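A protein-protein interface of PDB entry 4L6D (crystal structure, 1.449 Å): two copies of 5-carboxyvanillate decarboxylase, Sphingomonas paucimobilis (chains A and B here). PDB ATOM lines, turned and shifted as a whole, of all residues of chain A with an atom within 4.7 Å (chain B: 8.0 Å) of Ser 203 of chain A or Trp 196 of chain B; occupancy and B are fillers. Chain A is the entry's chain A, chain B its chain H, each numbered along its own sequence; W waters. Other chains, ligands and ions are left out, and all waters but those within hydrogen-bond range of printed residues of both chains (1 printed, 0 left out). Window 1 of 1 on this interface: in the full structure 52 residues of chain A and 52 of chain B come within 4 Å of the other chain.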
ATOM      1  N   GLY A 199     -28.010  -0.302  28.422  1.00  0.00           N
ATOM      2  CA  GLY A 199     -27.984  -0.933  27.113  1.00  0.00           C
ATOM      3  C   GLY A 199     -28.519  -2.348  27.124  1.00  0.00           C
ATOM      4  O   GLY A 199     -29.217  -2.761  26.195  1.00  0.00           O
ATOM      5  N   ILE A 200     -28.194  -3.100  28.164  1.00  0.00           N
ATOM      6  CA  ILE A 200     -28.681  -4.474  28.263  1.00  0.00           C
ATOM      7  C   ILE A 200     -30.201  -4.514  28.452  1.00  0.00           C
ATOM      8  O   ILE A 200     -30.902  -5.275  27.777  1.00  0.00           O
ATOM      9  CB  ILE A 200     -27.990  -5.229  29.405  1.00  0.00           C
ATOM     10  CG1 ILE A 200     -26.468  -5.266  29.203  1.00  0.00           C
ATOM     11  CG2 ILE A 200     -28.560  -6.637  29.513  1.00  0.00           C
ATOM     12  CD1 ILE A 200     -26.044  -5.862  27.867  1.00  0.00           C
ATOM     13  N   GLU A 201     -30.704  -3.673  29.350  1.00  0.00           N
ATOM     14  CA  GLU A 201     -32.135  -3.566  29.597  1.00  0.00           C
ATOM     15  C   GLU A 201     -32.921  -3.198  28.337  1.00  0.00           C
ATOM     16  O   GLU A 201     -33.899  -3.875  27.988  1.00  0.00           O
ATOM     17  CB  GLU A 201     -32.362  -2.533  30.715  1.00  0.00           C
ATOM     18  CG  GLU A 201     -33.755  -1.919  30.784  1.00  0.00           C
ATOM     19  CD  GLU A 201     -34.843  -2.905  31.166  1.00  0.00           C
ATOM     20  OE1 GLU A 201     -34.546  -3.968  31.765  1.00  0.00           O
ATOM     21  OE2 GLU A 201     -36.007  -2.598  30.840  1.00  0.00           O
ATOM     22  N   THR A 202     -32.462  -2.157  27.641  1.00  0.00           N
ATOM     23  CA  THR A 202     -33.212  -1.590  26.525  1.00  0.00           C
ATOM     24  C   THR A 202     -33.138  -2.483  25.290  1.00  0.00           C
ATOM     25  O   THR A 202     -34.151  -2.705  24.615  1.00  0.00           O
ATOM     26  CB  THR A 202     -32.708  -0.174  26.207  1.00  0.00           C
ATOM     27  OG1 THR A 202     -32.675   0.582  27.423  1.00  0.00           O
ATOM     28  CG2 THR A 202     -33.647   0.535  25.236  1.00  0.00           C
ATOM     29  N   SER A 203     -31.945  -3.005  24.997  1.00  0.00           N
ATOM     30  CA  SER A 203     -31.786  -3.902  23.859  1.00  0.00           C
ATOM     31  C   SER A 203     -32.579  -5.183  24.065  1.00  0.00           C
ATOM     32  O   SER A 203     -33.182  -5.695  23.122  1.00  0.00           O
ATOM     33  CB  SER A 203     -30.314  -4.230  23.570  1.00  0.00           C
ATOM     34  OG  SER A 203     -29.694  -4.872  24.672  1.00  0.00           O
ATOM     35  N   THR A 204     -32.580  -5.714  25.283  1.00  0.00           N
ATOM     36  CA  THR A 204     -33.329  -6.947  25.534  1.00  0.00           C
ATOM     37  C   THR A 204     -34.832  -6.740  25.341  1.00  0.00           C
ATOM     38  O   THR A 204     -35.507  -7.587  24.772  1.00  0.00           O
ATOM     39  CB  THR A 204     -32.998  -7.531  26.914  1.00  0.00           C
ATOM     40  OG1 THR A 204     -31.599  -7.858  26.961  1.00  0.00           O
ATOM     41  CG2 THR A 204     -33.811  -8.787  27.192  1.00  0.00           C
ATOM     42  N   ASN A 205     -35.340  -5.604  25.806  1.00  0.00           N
ATOM     43  CA  ASN A 205     -36.727  -5.225  25.571  1.00  0.00           C
ATOM     44  C   ASN A 205     -37.015  -5.259  24.065  1.00  0.00           C
ATOM     45  O   ASN A 205     -37.932  -5.948  23.599  1.00  0.00           O
ATOM     46  CB  ASN A 205     -36.961  -3.822  26.148  1.00  0.00           C
ATOM     47  CG  ASN A 205     -38.440  -3.497  26.364  1.00  0.00           C
ATOM     48  OD1 ASN A 205     -39.327  -4.173  25.852  1.00  0.00           O
ATOM     49  ND2 ASN A 205     -38.696  -2.444  27.146  1.00  0.00           N
ATOM     50  N   ALA A 206     -36.192  -4.560  23.288  1.00  0.00           N
ATOM     51  CA  ALA A 206     -36.420  -4.493  21.852  1.00  0.00           C
ATOM     52  C   ALA A 206     -36.324  -5.849  21.148  1.00  0.00           C
ATOM     53  O   ALA A 206     -37.099  -6.133  20.221  1.00  0.00           O
ATOM     54  CB  ALA A 206     -35.472  -3.481  21.207  1.00  0.00           C
ATOM     55  N   VAL A 207     -35.366  -6.677  21.561  1.00  0.00           N
ATOM     56  CA  VAL A 207     -35.253  -8.003  20.962  1.00  0.00           C
ATOM     57  C   VAL A 207     -36.499  -8.850  21.263  1.00  0.00           C
ATOM     58  O   VAL A 207     -37.000  -9.554  20.386  1.00  0.00           O
ATOM     59  CB  VAL A 207     -33.954  -8.707  21.408  1.00  0.00           C
ATOM     60  CG1 VAL A 207     -33.952 -10.176  20.995  1.00  0.00           C
ATOM     61  CG2 VAL A 207     -32.757  -7.983  20.813  1.00  0.00           C
ATOM     62  N   GLU A 230     -28.534   0.732  20.909  1.00  0.00           N
ATOM     63  CA  GLU A 230     -28.302  -0.183  22.032  1.00  0.00           C
ATOM     64  C   GLU A 230     -27.588  -1.450  21.573  1.00  0.00           C
ATOM     65  O   GLU A 230     -27.827  -2.539  22.092  1.00  0.00           O
ATOM     66  CB  GLU A 230     -29.606  -0.502  22.796  1.00  0.00           C
ATOM     67  CG  GLU A 230     -30.454   0.726  23.144  1.00  0.00           C
ATOM     68  CD  GLU A 230     -29.814   1.642  24.180  1.00  0.00           C
ATOM     69  OE1 GLU A 230     -28.720   1.323  24.686  1.00  0.00           O
ATOM     70  OE2 GLU A 230     -30.419   2.690  24.478  1.00  0.00           O
ATOM     71  N   ILE A 232     -27.893  -3.276  19.062  1.00  0.00           N
ATOM     72  CA  ILE A 232     -28.590  -4.205  18.172  1.00  0.00           C
ATOM     73  C   ILE A 232     -28.046  -4.197  16.717  1.00  0.00           C
ATOM     74  O   ILE A 232     -27.948  -5.261  16.091  1.00  0.00           O
ATOM     75  CB  ILE A 232     -30.127  -4.060  18.253  1.00  0.00           C
ATOM     76  CG1 ILE A 232     -30.602  -4.451  19.659  1.00  0.00           C
ATOM     77  CG2 ILE A 232     -30.806  -4.903  17.186  1.00  0.00           C
ATOM     78  CD1 ILE A 232     -32.013  -4.029  19.963  1.00  0.00           C
ATOM     79  N   TRP A 235     -25.454  -6.838  16.232  1.00  0.00           N
ATOM     80  CA  TRP A 235     -25.887  -8.236  16.382  1.00  0.00           C
ATOM     81  C   TRP A 235     -26.777  -8.774  15.255  1.00  0.00           C
ATOM     82  O   TRP A 235     -27.265  -9.904  15.347  1.00  0.00           O
ATOM     83  CB  TRP A 235     -26.659  -8.421  17.690  1.00  0.00           C
ATOM     84  CG  TRP A 235     -25.874  -8.320  18.975  1.00  0.00           C
ATOM     85  CD1 TRP A 235     -25.845  -7.265  19.852  1.00  0.00           C
ATOM     86  CD2 TRP A 235     -25.055  -9.344  19.561  1.00  0.00           C
ATOM     87  NE1 TRP A 235     -25.048  -7.567  20.928  1.00  0.00           N
ATOM     88  CE2 TRP A 235     -24.562  -8.838  20.785  1.00  0.00           C
ATOM     89  CE3 TRP A 235     -24.694 -10.637  19.170  1.00  0.00           C
ATOM     90  CZ2 TRP A 235     -23.715  -9.570  21.611  1.00  0.00           C
ATOM     91  CZ3 TRP A 235     -23.842 -11.370  19.999  1.00  0.00           C
ATOM     92  CH2 TRP A 235     -23.368 -10.831  21.209  1.00  0.00           C
ATOM     93  N   LEU A 239     -28.599 -12.546  15.079  1.00  0.00           N
ATOM     94  CA  LEU A 239     -30.041 -12.595  15.313  1.00  0.00           C
ATOM     95  C   LEU A 239     -30.734 -13.321  14.161  1.00  0.00           C
ATOM     96  O   LEU A 239     -31.593 -14.173  14.387  1.00  0.00           O
ATOM     97  CB  LEU A 239     -30.610 -11.180  15.466  1.00  0.00           C
ATOM     98  CG  LEU A 239     -30.318 -10.489  16.804  1.00  0.00           C
ATOM     99  CD1 LEU A 239     -30.584  -9.001  16.682  1.00  0.00           C
ATOM    100  CD2 LEU A 239     -31.179 -11.091  17.912  1.00  0.00           C
ATOM    101  N   ARG B 176     -22.412 -19.594  27.985  1.00  0.00           N
ATOM    102  CA  ARG B 176     -23.415 -20.582  28.360  1.00  0.00           C
ATOM    103  C   ARG B 176     -24.681 -19.752  28.571  1.00  0.00           C
ATOM    104  O   ARG B 176     -24.659 -18.536  28.373  1.00  0.00           O
ATOM    105  CB  ARG B 176     -23.029 -21.350  29.622  1.00  0.00           C
ATOM    106  CG  ARG B 176     -22.868 -20.488  30.861  1.00  0.00           C
ATOM    107  CD  ARG B 176     -22.460 -21.323  32.072  1.00  0.00           C
ATOM    108  NE  ARG B 176     -23.542 -22.163  32.564  1.00  0.00           N
ATOM    109  CZ  ARG B 176     -23.507 -22.806  33.727  1.00  0.00           C
ATOM    110  NH1 ARG B 176     -22.435 -22.707  34.501  1.00  0.00           N
ATOM    111  NH2 ARG B 176     -24.535 -23.549  34.113  1.00  0.00           N
ATOM    112  N   PRO B 178     -27.675 -17.568  30.157  1.00  0.00           N
ATOM    113  CA  PRO B 178     -27.805 -16.602  31.250  1.00  0.00           C
ATOM    114  C   PRO B 178     -27.899 -17.259  32.622  1.00  0.00           C
ATOM    115  O   PRO B 178     -28.681 -18.197  32.837  1.00  0.00           O
ATOM    116  CB  PRO B 178     -29.112 -15.889  30.900  1.00  0.00           C
ATOM    117  CG  PRO B 178     -29.037 -15.811  29.387  1.00  0.00           C
ATOM    118  CD  PRO B 178     -28.372 -17.106  28.941  1.00  0.00           C
ATOM    119  N   ILE B 182     -29.871 -13.364  35.916  1.00  0.00           N
ATOM    120  CA  ILE B 182     -30.516 -12.678  34.795  1.00  0.00           C
ATOM    121  C   ILE B 182     -31.451 -13.553  33.965  1.00  0.00           C
ATOM    122  O   ILE B 182     -32.069 -13.065  33.018  1.00  0.00           O
ATOM    123  CB  ILE B 182     -29.473 -12.048  33.830  1.00  0.00           C
ATOM    124  CG1 ILE B 182     -28.511 -13.115  33.296  1.00  0.00           C
ATOM    125  CG2 ILE B 182     -28.690 -10.935  34.527  1.00  0.00           C
ATOM    126  CD1 ILE B 182     -27.694 -12.659  32.091  1.00  0.00           C
ATOM    127  N   ALA B 185     -35.453 -13.136  32.152  1.00  0.00           N
ATOM    128  CA  ALA B 185     -35.798 -12.398  30.936  1.00  0.00           C
ATOM    129  C   ALA B 185     -35.472 -13.171  29.660  1.00  0.00           C
ATOM    130  O   ALA B 185     -35.670 -12.663  28.549  1.00  0.00           O
ATOM    131  CB  ALA B 185     -35.093 -11.046  30.923  1.00  0.00           C
ATOM    132  N   PHE B 186     -34.961 -14.391  29.820  1.00  0.00           N
ATOM    133  CA  PHE B 186     -34.468 -15.178  28.688  1.00  0.00           C
ATOM    134  C   PHE B 186     -35.174 -16.526  28.555  1.00  0.00           C
ATOM    135  O   PHE B 186     -34.642 -17.452  27.947  1.00  0.00           O
ATOM    136  CB  PHE B 186     -32.947 -15.365  28.798  1.00  0.00           C
ATOM    137  CG  PHE B 186     -32.182 -14.062  28.802  1.00  0.00           C
ATOM    138  CD1 PHE B 186     -31.974 -13.364  29.981  1.00  0.00           C
ATOM    139  CD2 PHE B 186     -31.697 -13.524  27.621  1.00  0.00           C
ATOM    140  CE1 PHE B 186     -31.290 -12.144  29.987  1.00  0.00           C
ATOM    141  CE2 PHE B 186     -31.014 -12.307  27.615  1.00  0.00           C
ATOM    142  CZ  PHE B 186     -30.806 -11.618  28.811  1.00  0.00           C
ATOM    143  N   ASP B 188     -38.111 -16.928  27.043  1.00  0.00           N
ATOM    144  CA  ASP B 188     -39.042 -16.909  25.913  1.00  0.00           C
ATOM    145  C   ASP B 188     -38.346 -16.816  24.562  1.00  0.00           C
ATOM    146  O   ASP B 188     -37.240 -16.300  24.465  1.00  0.00           O
ATOM    147  CB  ASP B 188     -40.019 -15.742  26.059  1.00  0.00           C
ATOM    148  CG  ASP B 188     -40.948 -15.918  27.234  1.00  0.00           C
ATOM    149  OD1 ASP B 188     -41.674 -16.933  27.256  1.00  0.00           O
ATOM    150  OD2 ASP B 188     -40.941 -15.060  28.144  1.00  0.00           O
ATOM    151  N   TYR B 189     -39.017 -17.316  23.524  1.00  0.00           N
ATOM    152  CA  TYR B 189     -38.583 -17.146  22.133  1.00  0.00           C
ATOM    153  C   TYR B 189     -37.175 -17.679  21.862  1.00  0.00           C
ATOM    154  O   TYR B 189     -36.483 -17.186  20.976  1.00  0.00           O
ATOM    155  CB  TYR B 189     -38.686 -15.669  21.695  1.00  0.00           C
ATOM    156  CG  TYR B 189     -39.876 -14.931  22.274  1.00  0.00           C
ATOM    157  CD1 TYR B 189     -41.174 -15.397  22.081  1.00  0.00           C
ATOM    158  CD2 TYR B 189     -39.707 -13.765  23.012  1.00  0.00           C
ATOM    159  CE1 TYR B 189     -42.268 -14.728  22.622  1.00  0.00           C
ATOM    160  CE2 TYR B 189     -40.790 -13.093  23.553  1.00  0.00           C
ATOM    161  CZ  TYR B 189     -42.067 -13.575  23.360  1.00  0.00           C
ATOM    162  OH  TYR B 189     -43.152 -12.912  23.897  1.00  0.00           O
ATOM    163  N   GLY B 190     -36.750 -18.675  22.634  1.00  0.00           N
ATOM    164  CA  GLY B 190     -35.444 -19.285  22.449  1.00  0.00           C
ATOM    165  C   GLY B 190     -34.284 -18.393  22.874  1.00  0.00           C
ATOM    166  O   GLY B 190     -33.130 -18.641  22.523  1.00  0.00           O
ATOM    167  N   MET B 191     -34.588 -17.349  23.640  1.00  0.00           N
ATOM    168  CA  MET B 191     -33.563 -16.369  23.988  1.00  0.00           C
ATOM    169  C   MET B 191     -32.530 -16.881  24.991  1.00  0.00           C
ATOM    170  O   MET B 191     -31.544 -16.195  25.267  1.00  0.00           O
ATOM    171  CB  MET B 191     -34.208 -15.072  24.471  1.00  0.00           C
ATOM    172  CG  MET B 191     -34.935 -14.360  23.337  1.00  0.00           C
ATOM    173  SD  MET B 191     -35.885 -12.920  23.819  1.00  0.00           S
ATOM    174  CE  MET B 191     -34.598 -11.866  24.504  1.00  0.00           C
ATOM    175  N   ASN B 192     -32.736 -18.095  25.507  1.00  0.00           N
ATOM    176  CA  ASN B 192     -31.747 -18.725  26.379  1.00  0.00           C
ATOM    177  C   ASN B 192     -30.423 -18.937  25.663  1.00  0.00           C
ATOM    178  O   ASN B 192     -29.363 -19.007  26.288  1.00  0.00           O
ATOM    179  CB  ASN B 192     -32.266 -20.076  26.908  1.00  0.00           C
ATOM    180  CG  ASN B 192     -32.298 -21.161  25.835  1.00  0.00           C
ATOM    181  OD1 ASN B 192     -31.334 -21.921  25.655  1.00  0.00           O
ATOM    182  ND2 ASN B 192     -33.399 -21.230  25.109  1.00  0.00           N
ATOM    183  N   SER B 193     -30.486 -19.021  24.336  1.00  0.00           N
ATOM    184  CA  SER B 193     -29.413 -19.594  23.545  1.00  0.00           C
ATOM    185  C   SER B 193     -28.619 -18.540  22.769  1.00  0.00           C
ATOM    186  O   SER B 193     -28.589 -17.360  23.144  1.00  0.00           O
ATOM    187  CB  SER B 193     -30.004 -20.649  22.597  1.00  0.00           C
ATOM    188  OG  SER B 193     -28.995 -21.414  21.951  1.00  0.00           O
ATOM    189  N   ALA B 194     -27.977 -18.980  21.688  1.00  0.00           N
ATOM    190  CA  ALA B 194     -27.101 -18.135  20.876  1.00  0.00           C
ATOM    191  C   ALA B 194     -27.773 -16.879  20.321  1.00  0.00           C
ATOM    192  O   ALA B 194     -27.112 -15.850  20.105  1.00  0.00           O
ATOM    193  CB  ALA B 194     -26.499 -18.957  19.727  1.00  0.00           C
ATOM    194  N   ILE B 195     -29.080 -16.949  20.082  1.00  0.00           N
ATOM    195  CA  ILE B 195     -29.781 -15.812  19.486  1.00  0.00           C
ATOM    196  C   ILE B 195     -29.713 -14.537  20.343  1.00  0.00           C
ATOM    197  O   ILE B 195     -29.742 -13.436  19.803  1.00  0.00           O
ATOM    198  CB  ILE B 195     -31.238 -16.167  19.099  1.00  0.00           C
ATOM    199  CG1 ILE B 195     -31.798 -15.164  18.073  1.00  0.00           C
ATOM    200  CG2 ILE B 195     -32.146 -16.256  20.341  1.00  0.00           C
ATOM    201  CD1 ILE B 195     -33.174 -15.524  17.542  1.00  0.00           C
ATOM    202  N   TRP B 196     -29.606 -14.667  21.663  1.00  0.00           N
ATOM    203  CA  TRP B 196     -29.517 -13.460  22.497  1.00  0.00           C
ATOM    204  C   TRP B 196     -28.847 -13.657  23.856  1.00  0.00           C
ATOM    205  O   TRP B 196     -27.905 -12.949  24.206  1.00  0.00           O
ATOM    206  CB  TRP B 196     -30.889 -12.772  22.662  1.00  0.00           C
ATOM    207  CG  TRP B 196     -30.747 -11.366  23.167  1.00  0.00           C
ATOM    208  CD1 TRP B 196     -31.204 -10.868  24.358  1.00  0.00           C
ATOM    209  CD2 TRP B 196     -30.086 -10.278  22.505  1.00  0.00           C
ATOM    210  NE1 TRP B 196     -30.884  -9.534  24.469  1.00  0.00           N
ATOM    211  CE2 TRP B 196     -30.194  -9.146  23.349  1.00  0.00           C
ATOM    212  CE3 TRP B 196     -29.423 -10.147  21.276  1.00  0.00           C
ATOM    213  CZ2 TRP B 196     -29.644  -7.906  23.013  1.00  0.00           C
ATOM    214  CZ3 TRP B 196     -28.891  -8.916  20.936  1.00  0.00           C
ATOM    215  CH2 TRP B 196     -28.996  -7.811  21.807  1.00  0.00           C
ATOM    216  N   GLY B 197     -29.344 -14.611  24.630  1.00  0.00           N
ATOM    217  CA  GLY B 197     -28.849 -14.779  25.987  1.00  0.00           C
ATOM    218  C   GLY B 197     -27.363 -15.078  26.088  1.00  0.00           C
ATOM    219  O   GLY B 197     -26.698 -14.593  26.995  1.00  0.00           O
ATOM    220  N   TYR B 198     -26.830 -15.878  25.169  1.00  0.00           N
ATOM    221  CA  TYR B 198     -25.405 -16.219  25.203  1.00  0.00           C
ATOM    222  C   TYR B 198     -24.541 -14.955  25.203  1.00  0.00           C
ATOM    223  O   TYR B 198     -23.582 -14.827  25.980  1.00  0.00           O
ATOM    224  CB  TYR B 198     -25.022 -17.110  24.010  1.00  0.00           C
ATOM    225  CG  TYR B 198     -25.273 -18.585  24.221  1.00  0.00           C
ATOM    226  CD1 TYR B 198     -26.066 -19.035  25.264  1.00  0.00           C
ATOM    227  CD2 TYR B 198     -24.695 -19.531  23.371  1.00  0.00           C
ATOM    228  CE1 TYR B 198     -26.286 -20.397  25.461  1.00  0.00           C
ATOM    229  CE2 TYR B 198     -24.896 -20.886  23.556  1.00  0.00           C
ATOM    230  CZ  TYR B 198     -25.697 -21.312  24.601  1.00  0.00           C
ATOM    231  OH  TYR B 198     -25.912 -22.656  24.806  1.00  0.00           O
ATOM    232  N   GLY B 199     -24.898 -14.007  24.343  1.00  0.00           N
ATOM    233  CA  GLY B 199     -24.130 -12.782  24.231  1.00  0.00           C
ATOM    234  C   GLY B 199     -24.252 -11.881  25.451  1.00  0.00           C
ATOM    235  O   GLY B 199     -23.272 -11.279  25.888  1.00  0.00           O
ATOM    236  N   ILE B 200     -25.460 -11.776  25.987  1.00  0.00           N
ATOM    237  CA  ILE B 200     -25.689 -10.945  27.173  1.00  0.00           C
ATOM    238  C   ILE B 200     -24.962 -11.492  28.399  1.00  0.00           C
ATOM    239  O   ILE B 200     -24.299 -10.757  29.132  1.00  0.00           O
ATOM    240  CB  ILE B 200     -27.199 -10.794  27.486  1.00  0.00           C
ATOM    241  CG1 ILE B 200     -27.946 -10.181  26.296  1.00  0.00           C
ATOM    242  CG2 ILE B 200     -27.395  -9.960  28.749  1.00  0.00           C
ATOM    243  CD1 ILE B 200     -27.327  -8.882  25.792  1.00  0.00           C
ATOM    244  N   GLU B 201     -25.093 -12.795  28.614  1.00  0.00           N
ATOM    245  CA  GLU B 201     -24.427 -13.488  29.708  1.00  0.00           C
ATOM    246  C   GLU B 201     -22.913 -13.291  29.660  1.00  0.00           C
ATOM    247  O   GLU B 201     -22.295 -12.894  30.651  1.00  0.00           O
ATOM    248  CB  GLU B 201     -24.790 -14.980  29.630  1.00  0.00           C
ATOM    249  CG  GLU B 201     -23.877 -15.951  30.384  1.00  0.00           C
ATOM    250  CD  GLU B 201     -23.837 -15.736  31.877  1.00  0.00           C
ATOM    251  OE1 GLU B 201     -24.798 -15.173  32.447  1.00  0.00           O
ATOM    252  OE2 GLU B 201     -22.826 -16.149  32.485  1.00  0.00           O
ATOM    253  N   THR B 202     -22.325 -13.548  28.498  1.00  0.00           N
ATOM    254  CA  THR B 202     -20.871 -13.589  28.387  1.00  0.00           C
ATOM    255  C   THR B 202     -20.277 -12.189  28.415  1.00  0.00           C
ATOM    256  O   THR B 202     -19.261 -11.951  29.087  1.00  0.00           O
ATOM    257  CB  THR B 202     -20.450 -14.303  27.107  1.00  0.00           C
ATOM    258  OG1 THR B 202     -21.130 -15.562  27.041  1.00  0.00           O
ATOM    259  CG2 THR B 202     -18.942 -14.537  27.080  1.00  0.00           C
ATOM    260  N   SER B 203     -20.928 -11.253  27.726  1.00  0.00           N
ATOM    261  CA  SER B 203     -20.421  -9.887  27.715  1.00  0.00           C
ATOM    262  C   SER B 203     -20.531  -9.267  29.107  1.00  0.00           C
ATOM    263  O   SER B 203     -19.639  -8.544  29.537  1.00  0.00           O
ATOM    264  CB  SER B 203     -21.146  -9.024  26.686  1.00  0.00           C
ATOM    265  OG  SER B 203     -22.522  -8.886  26.998  1.00  0.00           O
ATOM    266  N   GLU B 230     -18.509 -10.640  21.708  1.00  0.00           N
ATOM    267  CA  GLU B 230     -19.788 -10.517  22.403  1.00  0.00           C
ATOM    268  C   GLU B 230     -20.272  -9.067  22.413  1.00  0.00           C
ATOM    269  O   GLU B 230     -20.874  -8.611  23.388  1.00  0.00           O
ATOM    270  CB  GLU B 230     -19.722 -11.108  23.822  1.00  0.00           C
ATOM    271  CG  GLU B 230     -19.114 -12.525  23.874  1.00  0.00           C
ATOM    272  CD  GLU B 230     -19.971 -13.603  23.205  1.00  0.00           C
ATOM    273  OE1 GLU B 230     -21.095 -13.320  22.731  1.00  0.00           O
ATOM    274  OE2 GLU B 230     -19.490 -14.760  23.162  1.00  0.00           O
ATOM    275  N   ALA B 231     -19.983  -8.373  21.311  1.00  0.00           N
ATOM    276  CA  ALA B 231     -20.332  -6.966  21.061  1.00  0.00           C
ATOM    277  C   ALA B 231     -19.616  -5.931  21.914  1.00  0.00           C
ATOM    278  O   ALA B 231     -19.843  -4.731  21.717  1.00  0.00           O
ATOM    279  CB  ALA B 231     -21.861  -6.717  21.092  1.00  0.00           C
ATOM    280  N   TRP B 235     -19.210  -1.247  22.130  1.00  0.00           N
ATOM    281  CA  TRP B 235     -19.532  -0.409  23.283  1.00  0.00           C
ATOM    282  C   TRP B 235     -18.339   0.342  23.882  1.00  0.00           C
ATOM    283  O   TRP B 235     -18.484   0.991  24.917  1.00  0.00           O
ATOM    284  CB  TRP B 235     -20.113  -1.285  24.401  1.00  0.00           C
ATOM    285  CG  TRP B 235     -21.507  -1.841  24.186  1.00  0.00           C
ATOM    286  CD1 TRP B 235     -21.841  -3.135  23.865  1.00  0.00           C
ATOM    287  CD2 TRP B 235     -22.742  -1.131  24.331  1.00  0.00           C
ATOM    288  NE1 TRP B 235     -23.212  -3.262  23.798  1.00  0.00           N
ATOM    289  CE2 TRP B 235     -23.785  -2.050  24.094  1.00  0.00           C
ATOM    290  CE3 TRP B 235     -23.067   0.194  24.649  1.00  0.00           C
ATOM    291  CZ2 TRP B 235     -25.129  -1.678  24.156  1.00  0.00           C
ATOM    292  CZ3 TRP B 235     -24.403   0.562  24.712  1.00  0.00           C
ATOM    293  CH2 TRP B 235     -25.417  -0.373  24.459  1.00  0.00           C
HETATM  294  O   HOH W   1     -24.581  -5.785  23.167  1.00  0.00           O
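The backbone carbonyl oxygen of Gly 199 of chain A is in hydrogen-bond range of the side-chain hydroxyl of Ser 203 of chain A (2.6 Å). OG of Ser 203 of chain A lies within hydrogen-bond range of O of Ile 200 of chain A. O of Ile 200 of chain A is in hydrogen-bond range of OG1 of Thr 204 of chain A. The backbone carbonyl oxygen of Met 191 of chain B lies within hydrogen-bond range of the backbone NH of Gly 197 of chain B, at 2.8 Å. O of Gly 199 of chain B is in hydrogen-bond range of OG of Ser 203 of chain B. The backbone carbonyl oxygen (O) of Ile 200 of chain B lies within hydrogen-bond range of the side-chain hydroxyl (OG) of Ser 203 of chain B, 3.3 Å away.
Of the printed residues of chain B, Gly 199 of chain A touches Trp 235 (3.7 Å). Ser 203 of chain A touches one residue of chain B. Ala 206 of chain A touches none of the printed residues of chain B. Of the printed residues of chain A, Trp 196 of chain B touches Ser 203, Thr 204, Val 207, Trp 235 and Leu 239. Gly 197 of chain B touches none of the printed residues of chain A. Printed residues of chain A within 4 Å of Trp 235 of chain B: Gly 199 and Glu 230. The nearest residue of chain A that does not touch Trp 196 of chain B is Ile 232 of chain A (4.3 Å). The nearest printed residue of chain A that does not touch Trp 235 of chain B is Ile 200 of chain A (5.2 Å).
Gly 199 of chain A touches Trp 235 of chain B, and with the chains exchanged Trp 235 of chain A touches Gly 199 of chain B. Ile 200 of chain A touches its own counterpart, Ile 200 of chain B. Glu 230 of chain A touches Trp 235 of chain B, and with the chains exchanged Trp 235 of chain A touches Glu 230 of chain B. Positions printed for both chains: 199, 200, 201, 202, 203, 230 and 235. Of the 13 pairs that touch across the chains among the printed residues, 5 have their exchanged pair printed and touching as well.
Among the printed residues, pairs that only touch across the chains: Gly 199 of chain A with Trp 235 of chain B, Ile 200 of chain A with Ile 200 of chain B, Ser 203 of chain A with Trp 196 of chain B, Val 207 of chain A with Met 191 of chain B, Val 207 of chain A with Trp 196 of chain B, Glu 230 of chain A with Trp 235 of chain B, Trp 235 of chain A with Trp 196 of chain B, Trp 235 of chain A with Gly 199 of chain B, Trp 235 of chain A with Glu 230 of chain B, Trp 235 of chain A with Ala 231 of chain B, Leu 239 of chain A with Ile 195 of chain B and Leu 239 of chain A with Trp 196 of chain B.
Water W1 bridges the indole nitrogen (NE1) of Trp 235 of chain A (2.9 Å) and the indole nitrogen (NE1) of Trp 235 of chain B (2.9 Å).
Hydrophobic or aromatic side chains of chain A within 4 Å of the printed part of chain B: Ile 200, Val 207, Trp 235 and Leu 239. Hydrophobic or aromatic side chains of chain B within 4 Å of the printed part of chain A: Met 191, Ile 195, Trp 196, Ile 200, Ala 231 and Trp 235. Along chain B the printed residues that touch a printed residue of chain A span positions 191 to 235.
The indole nitrogen (NE1) of Trp 196 of chain B is in hydrogen-bond range of the side-chain hydroxyl (OG1) of Thr 204 of chain A (3.1 Å).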
